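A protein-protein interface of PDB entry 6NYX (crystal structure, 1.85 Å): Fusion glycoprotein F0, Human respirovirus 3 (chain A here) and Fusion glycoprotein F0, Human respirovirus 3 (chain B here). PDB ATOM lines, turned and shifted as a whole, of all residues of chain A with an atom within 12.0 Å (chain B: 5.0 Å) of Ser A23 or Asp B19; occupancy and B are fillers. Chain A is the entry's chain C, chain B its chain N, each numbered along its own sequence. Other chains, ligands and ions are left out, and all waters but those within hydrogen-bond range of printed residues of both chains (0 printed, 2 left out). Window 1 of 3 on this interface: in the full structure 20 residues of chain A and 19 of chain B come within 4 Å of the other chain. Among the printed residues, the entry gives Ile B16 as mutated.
The side-chain amide nitrogen of Asn A30 is in hydrogen-bond range of the side-chain carboxylate of Asp B19. The side-chain hydroxyl (OG) of Ser A26 lies within hydrogen-bond range of the side-chain carboxylate (OD2) of Asp B19, 2.9 Å away. The backbone carbonyl oxygen (O) of Ala A20 lies within hydrogen-bond range of the side-chain hydroxyl (OG) of Ser B23 (2.8 Å).
Of the 21 printed residues of chain A, 9 touch a printed residue of chain B. Hydrophobic or aromatic side chains of chain A within 4 Å of the printed part of chain B: Ala A20, Val A24 and Leu A31. Hydrophobic or aromatic side chains of chain B that line the printed part of chain A: Ile B16 and Trp B26. Among the printed residues, 17 pairs touch across the chains. Among the printed residues, no Asp or Glu carboxylate lies within 4 Å of a Lys or Arg side-chain nitrogen of the other chain.
Among the printed residues, pairs that only touch across the chains: Ser A27 with Asp B19 (3.2 Å), Val A24 with Ser B23 (3.3 Å), Lys A19 with Trp B26 (3.4 Å), Asn A30 with Ile B16 (3.4 Å), Asp A16 with Trp B26 (3.5 Å), Ser A23 with Asp B19 (3.5 Å), Ala A20 with Trp B26 (3.5 Å), Ser A23 with Trp B26 (3.5 Å), Leu A31 with Ile B16 (3.6 Å), Ser A27 with Ile B16 (3.6 Å), Ser A23 with Ser B23 (3.7 Å), Asn A30 with Lys B15 (3.7 Å), Ser A27 with Leu B20 (3.7 Å) and Ser A23 with Glu B22 (3.8 Å).
O of Ser A26 is in hydrogen-bond range of ND2 of Asn A30 (3.2 Å). The side-chain hydroxyl of Ser A27 lies within hydrogen-bond range of the backbone carbonyl oxygen of Ser A23, 3.5 Å away. The side-chain hydroxyl (OG) of Ser B18 is in hydrogen-bond range of the side-chain carboxylate (OE2) of Glu B22, at 3.3 Å. The backbone carbonyl oxygen of Lys A19 is in hydrogen-bond range of the side-chain hydroxyl of Ser A23, 3.4 Å away.
Of chain A, only Ser A23 (3.5 Å), Ser A26 (2.9 Å), Ser A27 (3.2 Å) and Asn A30 (3.1 Å) come within 4 Å of Asp B19. Ile B16 touches just these residues of chain A: Ser A27 (3.6 Å), Asn A30 (3.4 Å) and Leu A31 (3.6 Å). No residue of chain A comes within 4 Å of Ser B18. No residue of chain A comes within 4 Å of Glu B21. Ser B23 touches just these residues of chain A: Ala A20 (2.8 Å), Ser A23 (3.7 Å) and Val A24 (3.3 Å). Printed residues of chain B within 4 Å of Ser A26: Asp B19. Printed residues of chain B within 4 Å of Ser A27: Ile B16 (3.6 Å), Asp B19 (3.2 Å) and Leu B20 (3.7 Å). Lys B17 touches none of the printed residues of chain A. Arg A15 touches none of the printed residues of chain B. The nearest residue of chain A that does not touch Asp B19 is Val A24 (5.0 Å).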
ATOM      1  N   ILE A  14       9.687 -17.191 -12.101  1.00  0.00           N
ATOM      2  CA  ILE A  14       9.939 -16.017 -11.225  1.00  0.00           C
ATOM      3  C   ILE A  14      10.392 -14.833 -12.086  1.00  0.00           C
ATOM      4  O   ILE A  14       9.991 -13.757 -11.785  1.00  0.00           O
ATOM      5  CB  ILE A  14      10.917 -16.320 -10.080  1.00  0.00           C
ATOM      6  CG1 ILE A  14      10.458 -17.474  -9.208  1.00  0.00           C
ATOM      7  CG2 ILE A  14      11.145 -15.091  -9.246  1.00  0.00           C
ATOM      8  CD1 ILE A  14      11.548 -18.028  -8.347  1.00  0.00           C
ATOM      9  N   ARG A  15      11.192 -15.044 -13.124  1.00  0.00           N
ATOM     10  CA  ARG A  15      11.623 -13.937 -14.012  1.00  0.00           C
ATOM     11  C   ARG A  15      10.396 -13.266 -14.621  1.00  0.00           C
ATOM     12  O   ARG A  15      10.366 -12.081 -14.628  1.00  0.00           O
ATOM     13  CB  ARG A  15      12.516 -14.361 -15.177  1.00  0.00           C
ATOM     14  CG  ARG A  15      13.901 -14.757 -14.743  1.00  0.00           C
ATOM     15  CD  ARG A  15      14.937 -13.725 -15.097  1.00  0.00           C
ATOM     16  NE  ARG A  15      16.242 -14.338 -15.083  1.00  0.00           N
ATOM     17  CZ  ARG A  15      17.236 -13.947 -14.323  1.00  0.00           C
ATOM     18  NH1 ARG A  15      17.205 -12.756 -13.749  1.00  0.00           N
ATOM     19  NH2 ARG A  15      18.262 -14.752 -14.148  1.00  0.00           N
ATOM     20  N   ASP A  16       9.442 -14.060 -15.121  1.00  0.00           N
ATOM     21  CA  ASP A  16       8.203 -13.536 -15.754  1.00  0.00           C
ATOM     22  C   ASP A  16       7.413 -12.789 -14.667  1.00  0.00           C
ATOM     23  O   ASP A  16       6.942 -11.735 -14.913  1.00  0.00           O
ATOM     24  CB  ASP A  16       7.361 -14.628 -16.413  1.00  0.00           C
ATOM     25  CG  ASP A  16       7.974 -15.325 -17.616  1.00  0.00           C
ATOM     26  OD1 ASP A  16       8.683 -14.698 -18.340  1.00  0.00           O
ATOM     27  OD2 ASP A  16       7.686 -16.459 -17.810  1.00  0.00           O
ATOM     28  N   THR A  17       7.300 -13.355 -13.471  1.00  0.00           N
ATOM     29  CA  THR A  17       6.594 -12.678 -12.388  1.00  0.00           C
ATOM     30  C   THR A  17       7.271 -11.343 -12.089  1.00  0.00           C
ATOM     31  O   THR A  17       6.599 -10.327 -11.883  1.00  0.00           O
ATOM     32  CB  THR A  17       6.559 -13.553 -11.133  1.00  0.00           C
ATOM     33  OG1 THR A  17       5.814 -14.784 -11.369  1.00  0.00           O
ATOM     34  CG2 THR A  17       5.916 -12.821  -9.926  1.00  0.00           C
ATOM     35  N   ASN A  18       8.611 -11.296 -12.118  1.00  0.00           N
ATOM     36  CA  ASN A  18       9.304 -10.025 -11.810  1.00  0.00           C
ATOM     37  C   ASN A  18       9.033  -8.941 -12.860  1.00  0.00           C
ATOM     38  O   ASN A  18       8.815  -7.768 -12.516  1.00  0.00           O
ATOM     39  CB  ASN A  18      10.802 -10.271 -11.663  1.00  0.00           C
ATOM     40  CG  ASN A  18      11.170 -10.917 -10.321  1.00  0.00           C
ATOM     41  OD1 ASN A  18      10.357 -11.015  -9.428  1.00  0.00           O
ATOM     42  ND2 ASN A  18      12.409 -11.330 -10.186  1.00  0.00           N
ATOM     43  N   LYS A  19       8.933  -9.343 -14.115  1.00  0.00           N
ATOM     44  CA  LYS A  19       8.572  -8.444 -15.235  1.00  0.00           C
ATOM     45  C   LYS A  19       7.135  -7.953 -15.038  1.00  0.00           C
ATOM     46  O   LYS A  19       6.881  -6.802 -15.291  1.00  0.00           O
ATOM     47  CB  LYS A  19       8.801  -9.163 -16.554  1.00  0.00           C
ATOM     48  CG  LYS A  19      10.266  -9.302 -16.898  1.00  0.00           C
ATOM     49  CD  LYS A  19      10.520  -9.740 -18.289  1.00  0.00           C
ATOM     50  CE  LYS A  19      11.327 -11.006 -18.337  1.00  0.00           C
ATOM     51  NZ  LYS A  19      12.750 -10.696 -18.204  1.00  0.00           N
ATOM     52  N   ALA A  20       6.224  -8.819 -14.627  1.00  0.00           N
ATOM     53  CA  ALA A  20       4.873  -8.348 -14.322  1.00  0.00           C
ATOM     54  C   ALA A  20       4.885  -7.251 -13.259  1.00  0.00           C
ATOM     55  O   ALA A  20       4.123  -6.274 -13.345  1.00  0.00           O
ATOM     56  CB  ALA A  20       4.002  -9.525 -13.874  1.00  0.00           C
ATOM     57  N   VAL A  21       5.706  -7.417 -12.229  1.00  0.00           N
ATOM     58  CA  VAL A  21       5.800  -6.412 -11.194  1.00  0.00           C
ATOM     59  C   VAL A  21       6.436  -5.137 -11.767  1.00  0.00           C
ATOM     60  O   VAL A  21       6.027  -4.017 -11.430  1.00  0.00           O
ATOM     61  CB  VAL A  21       6.584  -6.968  -9.989  1.00  0.00           C
ATOM     62  CG1 VAL A  21       6.863  -5.883  -8.973  1.00  0.00           C
ATOM     63  CG2 VAL A  21       5.854  -8.177  -9.265  1.00  0.00           C
ATOM     64  N   GLN A  22       7.457  -5.274 -12.612  1.00  0.00           N
ATOM     65  CA  GLN A  22       8.065  -4.090 -13.231  1.00  0.00           C
ATOM     66  C   GLN A  22       7.042  -3.315 -14.059  1.00  0.00           C
ATOM     67  O   GLN A  22       7.011  -2.084 -14.029  1.00  0.00           O
ATOM     68  CB  GLN A  22       9.242  -4.495 -14.103  1.00  0.00           C
ATOM     69  CG  GLN A  22      10.454  -5.040 -13.354  1.00  0.00           C
ATOM     70  CD  GLN A  22      11.702  -5.133 -14.236  1.00  0.00           C
ATOM     71  OE1 GLN A  22      11.790  -5.969 -15.129  1.00  0.00           O
ATOM     72  NE2 GLN A  22      12.649  -4.240 -14.000  1.00  0.00           N
ATOM     73  N   SER A  23       6.175  -4.013 -14.794  1.00  0.00           N
ATOM     74  CA  SER A  23       5.095  -3.346 -15.527  1.00  0.00           C
ATOM     75  C   SER A  23       4.141  -2.623 -14.591  1.00  0.00           C
ATOM     76  O   SER A  23       3.645  -1.537 -14.908  1.00  0.00           O
ATOM     77  CB  SER A  23       4.304  -4.373 -16.374  1.00  0.00           C
ATOM     78  OG  SER A  23       5.065  -4.896 -17.439  1.00  0.00           O
ATOM     79  N   VAL A  24       3.851  -3.208 -13.428  1.00  0.00           N
ATOM     80  CA  VAL A  24       2.950  -2.552 -12.482  1.00  0.00           C
ATOM     81  C   VAL A  24       3.634  -1.332 -11.860  1.00  0.00           C
ATOM     82  O   VAL A  24       2.983  -0.325 -11.554  1.00  0.00           O
ATOM     83  CB  VAL A  24       2.507  -3.570 -11.407  1.00  0.00           C
ATOM     84  CG1 VAL A  24       2.047  -2.891 -10.098  1.00  0.00           C
ATOM     85  CG2 VAL A  24       1.353  -4.491 -11.916  1.00  0.00           C
ATOM     86  N   GLN A  25       4.937  -1.446 -11.571  1.00  0.00           N
ATOM     87  CA  GLN A  25       5.724  -0.292 -11.134  1.00  0.00           C
ATOM     88  C   GLN A  25       5.636   0.871 -12.127  1.00  0.00           C
ATOM     89  O   GLN A  25       5.446   2.018 -11.728  1.00  0.00           O
ATOM     90  CB  GLN A  25       7.183  -0.717 -10.954  1.00  0.00           C
ATOM     91  CG  GLN A  25       7.416  -1.539  -9.684  1.00  0.00           C
ATOM     92  CD  GLN A  25       8.760  -2.258  -9.676  1.00  0.00           C
ATOM     93  OE1 GLN A  25       9.508  -2.213 -10.622  1.00  0.00           O
ATOM     94  NE2 GLN A  25       9.048  -2.938  -8.584  1.00  0.00           N
ATOM     95  N   SER A  26       5.695   0.596 -13.414  1.00  0.00           N
ATOM     96  CA  SER A  26       5.540   1.633 -14.462  1.00  0.00           C
ATOM     97  C   SER A  26       4.146   2.271 -14.340  1.00  0.00           C
ATOM     98  O   SER A  26       4.032   3.458 -14.479  1.00  0.00           O
ATOM     99  CB  SER A  26       5.781   1.036 -15.789  1.00  0.00           C
ATOM    100  OG  SER A  26       5.643   1.992 -16.797  1.00  0.00           O
ATOM    101  N   SER A  27       3.125   1.461 -14.096  1.00  0.00           N
ATOM    102  CA  SER A  27       1.722   1.892 -13.903  1.00  0.00           C
ATOM    103  C   SER A  27       1.639   2.880 -12.750  1.00  0.00           C
ATOM    104  O   SER A  27       0.987   3.883 -12.877  1.00  0.00           O
ATOM    105  CB  SER A  27       0.825   0.729 -13.588  1.00  0.00           C
ATOM    106  OG  SER A  27       0.552   0.013 -14.756  1.00  0.00           O
ATOM    107  N   ILE A  28       2.256   2.530 -11.635  1.00  0.00           N
ATOM    108  CA  ILE A  28       2.211   3.390 -10.425  1.00  0.00           C
ATOM    109  C   ILE A  28       2.924   4.706 -10.735  1.00  0.00           C
ATOM    110  O   ILE A  28       2.406   5.742 -10.418  1.00  0.00           O
ATOM    111  CB  ILE A  28       2.742   2.629  -9.211  1.00  0.00           C
ATOM    112  CG1 ILE A  28       1.743   1.539  -8.833  1.00  0.00           C
ATOM    113  CG2 ILE A  28       3.041   3.549  -8.056  1.00  0.00           C
ATOM    114  CD1 ILE A  28       2.299   0.523  -7.935  1.00  0.00           C
ATOM    115  N   GLY A  29       4.052   4.654 -11.411  1.00  0.00           N
ATOM    116  CA  GLY A  29       4.757   5.884 -11.789  1.00  0.00           C
ATOM    117  C   GLY A  29       3.837   6.820 -12.562  1.00  0.00           C
ATOM    118  O   GLY A  29       3.793   7.983 -12.244  1.00  0.00           O
ATOM    119  N   ASN A  30       3.080   6.292 -13.518  1.00  0.00           N
ATOM    120  CA  ASN A  30       2.182   7.090 -14.339  1.00  0.00           C
ATOM    121  C   ASN A  30       0.936   7.510 -13.568  1.00  0.00           C
ATOM    122  O   ASN A  30       0.352   8.553 -13.874  1.00  0.00           O
ATOM    123  CB  ASN A  30       1.804   6.294 -15.576  1.00  0.00           C
ATOM    124  CG  ASN A  30       2.898   6.298 -16.635  1.00  0.00           C
ATOM    125  OD1 ASN A  30       3.453   7.325 -16.960  1.00  0.00           O
ATOM    126  ND2 ASN A  30       3.231   5.126 -17.145  1.00  0.00           N
ATOM    127  N   LEU A  31       0.510   6.731 -12.570  1.00  0.00           N
ATOM    128  CA  LEU A  31      -0.632   7.180 -11.773  1.00  0.00           C
ATOM    129  C   LEU A  31      -0.267   8.394 -10.928  1.00  0.00           C
ATOM    130  O   LEU A  31      -1.059   9.341 -10.824  1.00  0.00           O
ATOM    131  CB  LEU A  31      -1.136   6.052 -10.894  1.00  0.00           C
ATOM    132  CG  LEU A  31      -1.988   5.004 -11.617  1.00  0.00           C
ATOM    133  CD1 LEU A  31      -2.023   3.713 -10.850  1.00  0.00           C
ATOM    134  CD2 LEU A  31      -3.437   5.518 -11.814  1.00  0.00           C
ATOM    135  N   ILE A  32       0.956   8.415 -10.379  1.00  0.00           N
ATOM    136  CA  ILE A  32       1.464   9.600  -9.677  1.00  0.00           C
ATOM    137  C   ILE A  32       1.379  10.822 -10.572  1.00  0.00           C
ATOM    138  O   ILE A  32       1.004  11.920 -10.135  1.00  0.00           O
ATOM    139  CB  ILE A  32       2.930   9.387  -9.258  1.00  0.00           C
ATOM    140  CG1 ILE A  32       3.063   8.410  -8.154  1.00  0.00           C
ATOM    141  CG2 ILE A  32       3.570  10.730  -8.841  1.00  0.00           C
ATOM    142  CD1 ILE A  32       4.475   7.839  -8.069  1.00  0.00           C
ATOM    143  N   VAL A  33       1.790  10.663 -11.832  1.00  0.00           N
ATOM    144  CA  VAL A  33       1.771  11.782 -12.772  1.00  0.00           C
ATOM    145  C   VAL A  33       0.349  12.225 -13.049  1.00  0.00           C
ATOM    146  O   VAL A  33       0.073  13.430 -13.189  1.00  0.00           O
ATOM    147  CB  VAL A  33       2.485  11.414 -14.086  1.00  0.00           C
ATOM    148  CG1 VAL A  33       2.264  12.504 -15.130  1.00  0.00           C
ATOM    149  CG2 VAL A  33       3.968  11.132 -13.842  1.00  0.00           C
ATOM    150  N   ALA A  34      -0.569  11.262 -13.213  1.00  0.00           N
ATOM    151  CA  ALA A  34      -1.942  11.630 -13.506  1.00  0.00           C
ATOM    152  C   ALA A  34      -2.547  12.414 -12.350  1.00  0.00           C
ATOM    153  O   ALA A  34      -3.239  13.408 -12.572  1.00  0.00           O
ATOM    154  CB  ALA A  34      -2.767  10.396 -13.814  1.00  0.00           C
ATOM    155  N   LYS B  15      -1.393   5.249 -21.040  1.00  0.00           N
ATOM    156  CA  LYS B  15      -0.113   4.625 -20.702  1.00  0.00           C
ATOM    157  C   LYS B  15      -0.278   3.607 -19.588  1.00  0.00           C
ATOM    158  O   LYS B  15       0.279   2.502 -19.664  1.00  0.00           O
ATOM    159  CB  LYS B  15       0.919   5.674 -20.288  1.00  0.00           C
ATOM    160  CG  LYS B  15       1.283   6.626 -21.373  1.00  0.00           C
ATOM    161  CD  LYS B  15       2.355   7.623 -20.868  1.00  0.00           C
ATOM    162  CE  LYS B  15       3.657   6.935 -20.663  1.00  0.00           C
ATOM    163  NZ  LYS B  15       4.673   7.390 -21.681  1.00  0.00           N
ATOM    164  N   ILE B  16      -1.065   3.948 -18.576  1.00  0.00           N
ATOM    165  CA  ILE B  16      -1.323   3.033 -17.434  1.00  0.00           C
ATOM    166  C   ILE B  16      -2.032   1.777 -17.933  1.00  0.00           C
ATOM    167  O   ILE B  16      -1.618   0.720 -17.586  1.00  0.00           O
ATOM    168  CB  ILE B  16      -2.109   3.728 -16.318  1.00  0.00           C
ATOM    169  CG1 ILE B  16      -1.359   4.964 -15.829  1.00  0.00           C
ATOM    170  CG2 ILE B  16      -2.403   2.748 -15.199  1.00  0.00           C
ATOM    171  CD1 ILE B  16      -2.199   5.943 -15.124  1.00  0.00           C
ATOM    172  N   LYS B  17      -3.025   1.921 -18.792  1.00  0.00           N
ATOM    173  CA  LYS B  17      -3.756   0.761 -19.354  1.00  0.00           C
ATOM    174  C   LYS B  17      -2.793  -0.151 -20.114  1.00  0.00           C
ATOM    175  O   LYS B  17      -2.902  -1.325 -19.999  1.00  0.00           O
ATOM    176  CB  LYS B  17      -4.860   1.212 -20.300  1.00  0.00           C
ATOM    177  CG  LYS B  17      -5.926   2.035 -19.635  1.00  0.00           C
ATOM    178  CD  LYS B  17      -7.217   1.984 -20.351  1.00  0.00           C
ATOM    179  CE  LYS B  17      -7.393   3.100 -21.336  1.00  0.00           C
ATOM    180  NZ  LYS B  17      -8.696   3.777 -21.151  1.00  0.00           N
ATOM    181  N   SER B  18      -1.883   0.430 -20.872  1.00  0.00           N
ATOM    182  CA  SER B  18      -0.887  -0.314 -21.647  1.00  0.00           C
ATOM    183  C   SER B  18       0.017  -1.082 -20.673  1.00  0.00           C
ATOM    184  O   SER B  18       0.204  -2.224 -20.871  1.00  0.00           O
ATOM    185  CB  SER B  18      -0.158   0.624 -22.551  1.00  0.00           C
ATOM    186  OG  SER B  18       0.879  -0.042 -23.211  1.00  0.00           O
ATOM    187  N   ASP B  19       0.543  -0.450 -19.636  1.00  0.00           N
ATOM    188  CA  ASP B  19       1.424  -1.120 -18.674  1.00  0.00           C
ATOM    189  C   ASP B  19       0.670  -2.250 -17.975  1.00  0.00           C
ATOM    190  O   ASP B  19       1.221  -3.350 -17.727  1.00  0.00           O
ATOM    191  CB  ASP B  19       1.922  -0.109 -17.627  1.00  0.00           C
ATOM    192  CG  ASP B  19       2.835   0.993 -18.183  1.00  0.00           C
ATOM    193  OD1 ASP B  19       3.581   0.758 -19.158  1.00  0.00           O
ATOM    194  OD2 ASP B  19       2.841   2.124 -17.604  1.00  0.00           O
ATOM    195  N   LEU B  20      -0.593  -2.015 -17.679  1.00  0.00           N
ATOM    196  CA  LEU B  20      -1.453  -3.027 -17.024  1.00  0.00           C
ATOM    197  C   LEU B  20      -1.591  -4.244 -17.949  1.00  0.00           C
ATOM    198  O   LEU B  20      -1.397  -5.349 -17.497  1.00  0.00           O
ATOM    199  CB  LEU B  20      -2.801  -2.398 -16.680  1.00  0.00           C
ATOM    200  CG  LEU B  20      -3.725  -3.289 -15.866  1.00  0.00           C
ATOM    201  CD1 LEU B  20      -3.033  -3.756 -14.612  1.00  0.00           C
ATOM    202  CD2 LEU B  20      -5.017  -2.584 -15.528  1.00  0.00           C
ATOM    203  N   GLU B  21      -1.861  -4.032 -19.232  1.00  0.00           N
ATOM    204  CA  GLU B  21      -1.994  -5.141 -20.207  1.00  0.00           C
ATOM    205  C   GLU B  21      -0.672  -5.905 -20.293  1.00  0.00           C
ATOM    206  O   GLU B  21      -0.707  -7.125 -20.356  1.00  0.00           O
ATOM    207  CB  GLU B  21      -2.451  -4.646 -21.572  1.00  0.00           C
ATOM    208  CG  GLU B  21      -3.950  -4.458 -21.653  1.00  0.00           C
ATOM    209  CD  GLU B  21      -4.801  -5.567 -21.046  1.00  0.00           C
ATOM    210  OE1 GLU B  21      -4.775  -6.679 -21.576  1.00  0.00           O
ATOM    211  OE2 GLU B  21      -5.497  -5.307 -20.076  1.00  0.00           O
ATOM    212  N   GLU B  22       0.450  -5.206 -20.294  1.00  0.00           N
ATOM    213  CA  GLU B  22       1.774  -5.859 -20.359  1.00  0.00           C
ATOM    214  C   GLU B  22       1.953  -6.700 -19.087  1.00  0.00           C
ATOM    215  O   GLU B  22       2.442  -7.792 -19.164  1.00  0.00           O
ATOM    216  CB  GLU B  22       2.860  -4.810 -20.582  1.00  0.00           C
ATOM    217  CG  GLU B  22       2.694  -4.121 -21.926  1.00  0.00           C
ATOM    218  CD  GLU B  22       3.483  -2.848 -22.178  1.00  0.00           C
ATOM    219  OE1 GLU B  22       4.284  -2.477 -21.330  1.00  0.00           O
ATOM    220  OE2 GLU B  22       3.305  -2.269 -23.247  1.00  0.00           O
ATOM    221  N   SER B  23       1.541  -6.187 -17.946  1.00  0.00           N
ATOM    222  CA  SER B  23       1.669  -6.954 -16.701  1.00  0.00           C
ATOM    223  C   SER B  23       0.876  -8.256 -16.769  1.00  0.00           C
ATOM    224  O   SER B  23       1.361  -9.318 -16.339  1.00  0.00           O
ATOM    225  CB  SER B  23       1.191  -6.105 -15.527  1.00  0.00           C
ATOM    226  OG  SER B  23       1.498  -6.724 -14.280  1.00  0.00           O
ATOM    227  N   TRP B  26       2.754 -10.975 -18.738  1.00  0.00           N
ATOM    228  CA  TRP B  26       3.859 -11.604 -18.013  1.00  0.00           C
ATOM    229  C   TRP B  26       3.337 -12.594 -16.974  1.00  0.00           C
ATOM    230  O   TRP B  26       3.909 -13.671 -16.802  1.00  0.00           O
ATOM    231  CB  TRP B  26       4.786 -10.570 -17.342  1.00  0.00           C
ATOM    232  CG  TRP B  26       5.519  -9.659 -18.235  1.00  0.00           C
ATOM    233  CD1 TRP B  26       5.334  -8.303 -18.378  1.00  0.00           C
ATOM    234  CD2 TRP B  26       6.555 -10.016 -19.123  1.00  0.00           C
ATOM    235  NE1 TRP B  26       6.217  -7.810 -19.307  1.00  0.00           N
ATOM    236  CE2 TRP B  26       6.961  -8.855 -19.788  1.00  0.00           C
ATOM    237  CE3 TRP B  26       7.172 -11.215 -19.432  1.00  0.00           C
ATOM    238  CZ2 TRP B  26       7.962  -8.869 -20.740  1.00  0.00           C
ATOM    239  CZ3 TRP B  26       8.151 -11.235 -20.405  1.00  0.00           C
ATOM    240  CH2 TRP B  26       8.547 -10.076 -21.025  1.00  0.00           C
